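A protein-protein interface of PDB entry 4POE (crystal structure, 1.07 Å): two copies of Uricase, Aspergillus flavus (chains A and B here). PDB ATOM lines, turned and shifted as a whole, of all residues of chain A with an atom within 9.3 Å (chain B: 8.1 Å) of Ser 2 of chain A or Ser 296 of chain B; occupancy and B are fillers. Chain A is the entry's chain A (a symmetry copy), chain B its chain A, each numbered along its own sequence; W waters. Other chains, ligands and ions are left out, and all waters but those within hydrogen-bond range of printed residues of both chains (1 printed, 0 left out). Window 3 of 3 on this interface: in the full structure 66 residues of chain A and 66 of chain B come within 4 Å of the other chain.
Water W1 lies within hydrogen-bond range of the side-chain hydroxyl of Ser 2 of chain A (2.6 Å) and the backbone carbonyl oxygen of Glu 237 of chain B (2.8 Å).
Of the 15 printed residues of chain B, 7 touch a printed residue of chain A.
Hydrophobic or aromatic side chains of chain B within 4 Å of the printed part of chain A: Tyr 233, Leu 240 and Val 293.
Hydrophobic or aromatic side chains of chain A that line the printed part of chain B: Val 4.
Among the printed residues, 15 pairs touch across the chains.
Among the printed residues, no Asp or Glu carboxylate lies within 4 Å of a Lys or Arg side-chain nitrogen of the other chain.
O of Val 249 of chain B is in hydrogen-bond range of N of Val 293 of chain B (2.8 Å).
NH2 of Arg 295 of chain B sits at hydrogen-bond distance from O of Leu 240 of chain B, at 2.8 Å.
The backbone carbonyl oxygen of Ser 2 of chain A is in hydrogen-bond range of the side-chain hydroxyl of Tyr 233 of chain B, 3.2 Å away.
The side-chain hydroxyl of Ser 296 of chain B lies within hydrogen-bond range of the backbone NH of Ser 2 of chain A (3.4 Å).
The backbone NH (N) of Ser 296 of chain B lies within hydrogen-bond range of O of ACE 1 of chain A.
OH of Tyr 233 of chain B sits at hydrogen-bond distance from N of Ala 3 of chain A (3.4 Å).
O of Arg 295 of chain B lies within hydrogen-bond range of NZ of Lys 5 of chain A (3.2 Å).
O of Gly 294 of chain B lies within hydrogen-bond range of N of Ala 3 of chain A, at 3.0 Å.
O of ACE 1 of chain A touches CA of Arg 295 of chain B (3.6 Å).
Glu 237 of chain B touches Ser 2 of chain A (CA to OG, 3.6 Å).
Leu 240 of chain B touches Ser 2 of chain A.
Val 293 of chain B touches Ser 2 of chain A (CG1 to CB, 3.8 Å).
CA of Ser 2 of chain A touches O of Gly 294 of chain B (3.3 Å).
O of Ala 3 of chain A touches CA of Val 293 of chain B, at 3.4 Å.
CG2 of Val 4 of chain A touches CE1 of Tyr 233 of chain B, 3.6 Å away.
CG of Lys 5 of chain A touches N of Gly 294 of chain B, at 3.5 Å.
Tyr 233 of chain B touches Thr 48 of chain A (CZ to CG2, 3.7 Å).
ACE 1 of chain A touches two residues of chain B.
Of chain B, only Tyr 233, Glu 237, Leu 240, Val 293, Gly 294 and Ser 296 come within 4 Å of Ser 2 of chain A.
Of the printed residues of chain B, Thr 48 of chain A touches Tyr 233 (3.7 Å).
Met 235 of chain B touches none of the printed residues of chain A.
Ala 241 of chain B touches none of the printed residues of chain A.
Printed residues of chain A within 4 Å of Val 293 of chain B: Ser 2 and Ala 3.
The nearest residue of chain B that does not touch Ser 2 of chain A is Arg 295 of chain B (4.5 Å).
The nearest residue of chain A that does not touch Ser 296 of chain B is Ala 3 of chain A (4.1 Å).
No position is printed for both chains.
Of the 15 pairs that touch across the chains among the printed residues, none has its exchanged pair printed and touching as well.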
ATOM      1  C   ACE A   1     -19.396 -26.412 -10.931  1.00  0.00           C
ATOM      2  O   ACE A   1     -19.052 -25.814  -9.919  1.00  0.00           O
ATOM      3  CH3 ACE A   1     -19.643 -27.924 -10.923  1.00  0.00           C
ATOM      4  N   SER A   2     -19.533 -25.729 -11.904  1.00  0.00           N
ATOM      5  CA  SER A   2     -19.427 -24.278 -12.129  1.00  0.00           C
ATOM      6  C   SER A   2     -20.790 -23.706 -12.477  1.00  0.00           C
ATOM      7  O   SER A   2     -21.700 -24.380 -12.921  1.00  0.00           O
ATOM      8  CB  SER A   2     -18.446 -23.904 -13.239  1.00  0.00           C
ATOM      9  OG  SER A   2     -17.103 -24.195 -13.081  1.00  0.00           O
ATOM     10  N   ALA A   3     -20.934 -22.402 -12.277  1.00  0.00           N
ATOM     11  CA  ALA A   3     -22.115 -21.633 -12.537  1.00  0.00           C
ATOM     12  C   ALA A   3     -21.797 -20.178 -12.786  1.00  0.00           C
ATOM     13  O   ALA A   3     -20.861 -19.577 -12.272  1.00  0.00           O
ATOM     14  CB  ALA A   3     -23.079 -21.758 -11.382  1.00  0.00           C
ATOM     15  N   VAL A   4     -22.622 -19.542 -13.618  1.00  0.00           N
ATOM     16  CA  VAL A   4     -22.446 -18.114 -13.855  1.00  0.00           C
ATOM     17  C   VAL A   4     -22.915 -17.336 -12.647  1.00  0.00           C
ATOM     18  O   VAL A   4     -24.052 -17.469 -12.181  1.00  0.00           O
ATOM     19  CB  VAL A   4     -23.260 -17.690 -15.108  1.00  0.00           C
ATOM     20  CG1 VAL A   4     -23.247 -16.181 -15.277  1.00  0.00           C
ATOM     21  CG2 VAL A   4     -22.712 -18.400 -16.350  1.00  0.00           C
ATOM     22  N   LYS A   5     -22.052 -16.534 -12.045  1.00  0.00           N
ATOM     23  CA  LYS A   5     -22.394 -15.688 -10.913  1.00  0.00           C
ATOM     24  C   LYS A   5     -22.757 -14.280 -11.324  1.00  0.00           C
ATOM     25  O   LYS A   5     -23.567 -13.583 -10.676  1.00  0.00           O
ATOM     26  CB  LYS A   5     -21.191 -15.618  -9.943  1.00  0.00           C
ATOM     27  CG  LYS A   5     -20.756 -16.953  -9.421  1.00  0.00           C
ATOM     28  CD  LYS A   5     -21.795 -17.666  -8.536  1.00  0.00           C
ATOM     29  CE  LYS A   5     -21.362 -19.137  -8.307  1.00  0.00           C
ATOM     30  NZ  LYS A   5     -22.563 -20.004  -8.115  1.00  0.00           N
ATOM     31  N   THR A  48     -23.505 -21.160 -20.919  1.00  0.00           N
ATOM     32  CA  THR A  48     -23.377 -22.513 -20.407  1.00  0.00           C
ATOM     33  C   THR A  48     -23.839 -23.587 -21.396  1.00  0.00           C
ATOM     34  O   THR A  48     -23.430 -24.746 -21.272  1.00  0.00           O
ATOM     35  CB  THR A  48     -24.204 -22.755 -19.104  1.00  0.00           C
ATOM     36  OG1 THR A  48     -25.552 -22.417 -19.382  1.00  0.00           O
ATOM     37  CG2 THR A  48     -23.720 -21.850 -18.000  1.00  0.00           C
ATOM     38  N   LYS A  49     -24.694 -23.195 -22.372  1.00  0.00           N
ATOM     39  CA  LYS A  49     -25.327 -24.231 -23.222  1.00  0.00           C
ATOM     40  C   LYS A  49     -25.365 -23.791 -24.685  1.00  0.00           C
ATOM     41  O   LYS A  49     -26.138 -24.328 -25.469  1.00  0.00           O
ATOM     42  CB  LYS A  49     -26.745 -24.565 -22.782  1.00  0.00           C
ATOM     43  CG  LYS A  49     -27.026 -25.184 -21.456  1.00  0.00           C
ATOM     44  CD  LYS A  49     -26.468 -26.547 -21.181  1.00  0.00           C
ATOM     45  CE  LYS A  49     -27.140 -27.113 -19.907  1.00  0.00           C
ATOM     46  NZ  LYS A  49     -26.382 -28.302 -19.412  1.00  0.00           N
ATOM     47  N   TYR B 233     -16.755 -19.203 -21.017  1.00  0.00           N
ATOM     48  CA  TYR B 233     -17.242 -20.010 -19.917  1.00  0.00           C
ATOM     49  C   TYR B 233     -16.451 -21.286 -19.794  1.00  0.00           C
ATOM     50  O   TYR B 233     -16.098 -21.720 -18.660  1.00  0.00           O
ATOM     51  CB  TYR B 233     -18.752 -20.250 -20.107  1.00  0.00           C
ATOM     52  CG  TYR B 233     -19.308 -21.005 -18.895  1.00  0.00           C
ATOM     53  CD1 TYR B 233     -19.695 -20.312 -17.774  1.00  0.00           C
ATOM     54  CD2 TYR B 233     -19.441 -22.368 -18.947  1.00  0.00           C
ATOM     55  CE1 TYR B 233     -20.199 -21.006 -16.658  1.00  0.00           C
ATOM     56  CE2 TYR B 233     -19.934 -23.091 -17.841  1.00  0.00           C
ATOM     57  CZ  TYR B 233     -20.307 -22.347 -16.756  1.00  0.00           C
ATOM     58  OH  TYR B 233     -20.807 -23.012 -15.626  1.00  0.00           O
ATOM     59  N   LYS B 234     -16.095 -21.925 -20.910  1.00  0.00           N
ATOM     60  CA  LYS B 234     -15.291 -23.127 -20.890  1.00  0.00           C
ATOM     61  C   LYS B 234     -13.939 -22.855 -20.237  1.00  0.00           C
ATOM     62  O   LYS B 234     -13.400 -23.673 -19.506  1.00  0.00           O
ATOM     63  CB  LYS B 234     -15.125 -23.683 -22.299  1.00  0.00           C
ATOM     64  CG  LYS B 234     -16.443 -24.173 -22.880  1.00  0.00           C
ATOM     65  CD  LYS B 234     -16.289 -24.767 -24.269  1.00  0.00           C
ATOM     66  CE  LYS B 234     -17.649 -24.911 -24.926  1.00  0.00           C
ATOM     67  NZ  LYS B 234     -17.675 -25.634 -26.189  1.00  0.00           N
ATOM     68  N   MET B 235     -13.362 -21.694 -20.550  1.00  0.00           N
ATOM     69  CA  MET B 235     -12.060 -21.365 -19.950  1.00  0.00           C
ATOM     70  C   MET B 235     -12.167 -21.293 -18.440  1.00  0.00           C
ATOM     71  O   MET B 235     -11.365 -21.844 -17.677  1.00  0.00           O
ATOM     72  CB  MET B 235     -11.566 -20.030 -20.464  1.00  0.00           C
ATOM     73  CG  MET B 235     -11.289 -19.937 -21.945  1.00  0.00           C
ATOM     74  SD  MET B 235     -10.927 -18.265 -22.491  1.00  0.00           S
ATOM     75  CE  MET B 235     -10.599 -18.507 -24.232  1.00  0.00           C
ATOM     76  N   ALA B 236     -13.193 -20.566 -17.994  1.00  0.00           N
ATOM     77  CA  ALA B 236     -13.368 -20.341 -16.542  1.00  0.00           C
ATOM     78  C   ALA B 236     -13.594 -21.673 -15.858  1.00  0.00           C
ATOM     79  O   ALA B 236     -13.054 -21.864 -14.748  1.00  0.00           O
ATOM     80  CB  ALA B 236     -14.480 -19.356 -16.302  1.00  0.00           C
ATOM     81  N   GLU B 237     -14.425 -22.528 -16.420  1.00  0.00           N
ATOM     82  CA  GLU B 237     -14.766 -23.772 -15.727  1.00  0.00           C
ATOM     83  C   GLU B 237     -13.512 -24.604 -15.541  1.00  0.00           C
ATOM     84  O   GLU B 237     -13.325 -25.218 -14.468  1.00  0.00           O
ATOM     85  CB  GLU B 237     -15.826 -24.568 -16.435  1.00  0.00           C
ATOM     86  CG  GLU B 237     -16.838 -24.131 -17.431  1.00  0.00           C
ATOM     87  CD  GLU B 237     -17.471 -25.381 -18.048  1.00  0.00           C
ATOM     88  OE1 GLU B 237     -17.243 -25.615 -19.245  1.00  0.00           O
ATOM     89  OE2 GLU B 237     -18.152 -26.110 -17.285  1.00  0.00           O
ATOM     90  N   GLN B 238     -12.634 -24.626 -16.516  1.00  0.00           N
ATOM     91  CA  GLN B 238     -11.435 -25.442 -16.414  1.00  0.00           C
ATOM     92  C   GLN B 238     -10.488 -24.864 -15.380  1.00  0.00           C
ATOM     93  O   GLN B 238      -9.822 -25.609 -14.679  1.00  0.00           O
ATOM     94  CB  GLN B 238     -10.738 -25.480 -17.763  1.00  0.00           C
ATOM     95  CG  GLN B 238     -11.445 -26.396 -18.720  1.00  0.00           C
ATOM     96  CD  GLN B 238     -10.792 -26.224 -20.108  1.00  0.00           C
ATOM     97  OE1 GLN B 238      -9.666 -26.609 -20.341  1.00  0.00           O
ATOM     98  NE2 GLN B 238     -11.653 -25.696 -20.963  1.00  0.00           N
ATOM     99  N   ILE B 239     -10.356 -23.540 -15.291  1.00  0.00           N
ATOM    100  CA  ILE B 239      -9.444 -22.971 -14.285  1.00  0.00           C
ATOM    101  C   ILE B 239      -9.946 -23.311 -12.892  1.00  0.00           C
ATOM    102  O   ILE B 239      -9.165 -23.709 -12.006  1.00  0.00           O
ATOM    103  CB  ILE B 239      -9.274 -21.472 -14.530  1.00  0.00           C
ATOM    104  CG1 ILE B 239      -8.591 -21.209 -15.867  1.00  0.00           C
ATOM    105  CG2 ILE B 239      -8.514 -20.795 -13.401  1.00  0.00           C
ATOM    106  CD1 ILE B 239      -8.712 -19.834 -16.458  1.00  0.00           C
ATOM    107  N   LEU B 240     -11.263 -23.181 -12.670  1.00  0.00           N
ATOM    108  CA  LEU B 240     -11.796 -23.517 -11.341  1.00  0.00           C
ATOM    109  C   LEU B 240     -11.581 -24.967 -10.999  1.00  0.00           C
ATOM    110  O   LEU B 240     -11.318 -25.287  -9.815  1.00  0.00           O
ATOM    111  CB  LEU B 240     -13.288 -23.206 -11.309  1.00  0.00           C
ATOM    112  CG  LEU B 240     -13.644 -21.734 -11.248  1.00  0.00           C
ATOM    113  CD1 LEU B 240     -15.128 -21.523 -11.526  1.00  0.00           C
ATOM    114  CD2 LEU B 240     -13.295 -21.102  -9.894  1.00  0.00           C
ATOM    115  N   ALA B 241     -11.618 -25.848 -11.977  1.00  0.00           N
ATOM    116  CA  ALA B 241     -11.425 -27.289 -11.733  1.00  0.00           C
ATOM    117  C   ALA B 241      -9.972 -27.573 -11.366  1.00  0.00           C
ATOM    118  O   ALA B 241      -9.684 -28.601 -10.738  1.00  0.00           O
ATOM    119  CB  ALA B 241     -11.796 -28.139 -12.931  1.00  0.00           C
ATOM    120  N   GLU B 247     -11.893 -18.979  -5.880  1.00  0.00           N
ATOM    121  CA  GLU B 247     -13.339 -18.970  -5.704  1.00  0.00           C
ATOM    122  C   GLU B 247     -14.089 -18.574  -6.972  1.00  0.00           C
ATOM    123  O   GLU B 247     -15.136 -19.162  -7.251  1.00  0.00           O
ATOM    124  CB  GLU B 247     -13.678 -18.008  -4.572  1.00  0.00           C
ATOM    125  CG  GLU B 247     -13.218 -18.549  -3.227  1.00  0.00           C
ATOM    126  CD  GLU B 247     -13.626 -17.682  -2.065  1.00  0.00           C
ATOM    127  OE1 GLU B 247     -13.980 -16.506  -2.176  1.00  0.00           O
ATOM    128  OE2 GLU B 247     -13.523 -18.252  -0.918  1.00  0.00           O
ATOM    129  N   VAL B 249     -13.624 -16.940 -11.249  1.00  0.00           N
ATOM    130  CA  VAL B 249     -12.862 -16.528 -12.430  1.00  0.00           C
ATOM    131  C   VAL B 249     -13.695 -15.546 -13.246  1.00  0.00           C
ATOM    132  O   VAL B 249     -14.888 -15.796 -13.502  1.00  0.00           O
ATOM    133  CB  VAL B 249     -12.476 -17.696 -13.297  1.00  0.00           C
ATOM    134  CG1 VAL B 249     -11.774 -17.271 -14.591  1.00  0.00           C
ATOM    135  CG2 VAL B 249     -11.586 -18.671 -12.512  1.00  0.00           C
ATOM    136  N   VAL B 293     -17.606 -16.512 -13.079  1.00  0.00           N
ATOM    137  CA  VAL B 293     -17.973 -17.885 -12.909  1.00  0.00           C
ATOM    138  C   VAL B 293     -17.462 -18.322 -11.527  1.00  0.00           C
ATOM    139  O   VAL B 293     -16.303 -18.047 -11.154  1.00  0.00           O
ATOM    140  CB  VAL B 293     -17.371 -18.769 -14.001  1.00  0.00           C
ATOM    141  CG1 VAL B 293     -17.781 -20.207 -13.837  1.00  0.00           C
ATOM    142  CG2 VAL B 293     -17.800 -18.242 -15.400  1.00  0.00           C
ATOM    143  N   GLY B 294     -18.337 -19.025 -10.807  1.00  0.00           N
ATOM    144  CA  GLY B 294     -18.020 -19.484  -9.480  1.00  0.00           C
ATOM    145  C   GLY B 294     -18.430 -20.939  -9.398  1.00  0.00           C
ATOM    146  O   GLY B 294     -18.791 -21.560 -10.414  1.00  0.00           O
ATOM    147  N   ARG B 295     -18.343 -21.467  -8.212  1.00  0.00           N
ATOM    148  CA  ARG B 295     -18.578 -22.863  -7.924  1.00  0.00           C
ATOM    149  C   ARG B 295     -20.060 -23.076  -7.724  1.00  0.00           C
ATOM    150  O   ARG B 295     -20.657 -22.294  -6.996  1.00  0.00           O
ATOM    151  CB  ARG B 295     -17.706 -23.227  -6.691  1.00  0.00           C
ATOM    152  CG  ARG B 295     -16.210 -22.996  -7.007  1.00  0.00           C
ATOM    153  CD  ARG B 295     -15.288 -23.536  -5.886  1.00  0.00           C
ATOM    154  NE  ARG B 295     -13.846 -23.265  -6.269  1.00  0.00           N
ATOM    155  CZ  ARG B 295     -13.255 -24.009  -7.133  1.00  0.00           C
ATOM    156  NH1 ARG B 295     -13.820 -25.066  -7.728  1.00  0.00           N
ATOM    157  NH2 ARG B 295     -11.986 -23.820  -7.515  1.00  0.00           N
ATOM    158  N   SER B 296     -20.579 -24.112  -8.360  1.00  0.00           N
ATOM    159  CA  SER B 296     -21.984 -24.446  -8.173  1.00  0.00           C
ATOM    160  C   SER B 296     -22.150 -25.216  -6.849  1.00  0.00           C
ATOM    161  O   SER B 296     -21.264 -26.084  -6.621  1.00  0.00           O
ATOM    162  CB  SER B 296     -22.467 -25.265  -9.366  1.00  0.00           C
ATOM    163  OG  SER B 296     -21.743 -26.495  -9.414  1.00  0.00           O
HETATM  164  O   HOH W   1     -15.361 -26.123 -12.768  1.00  0.00           O
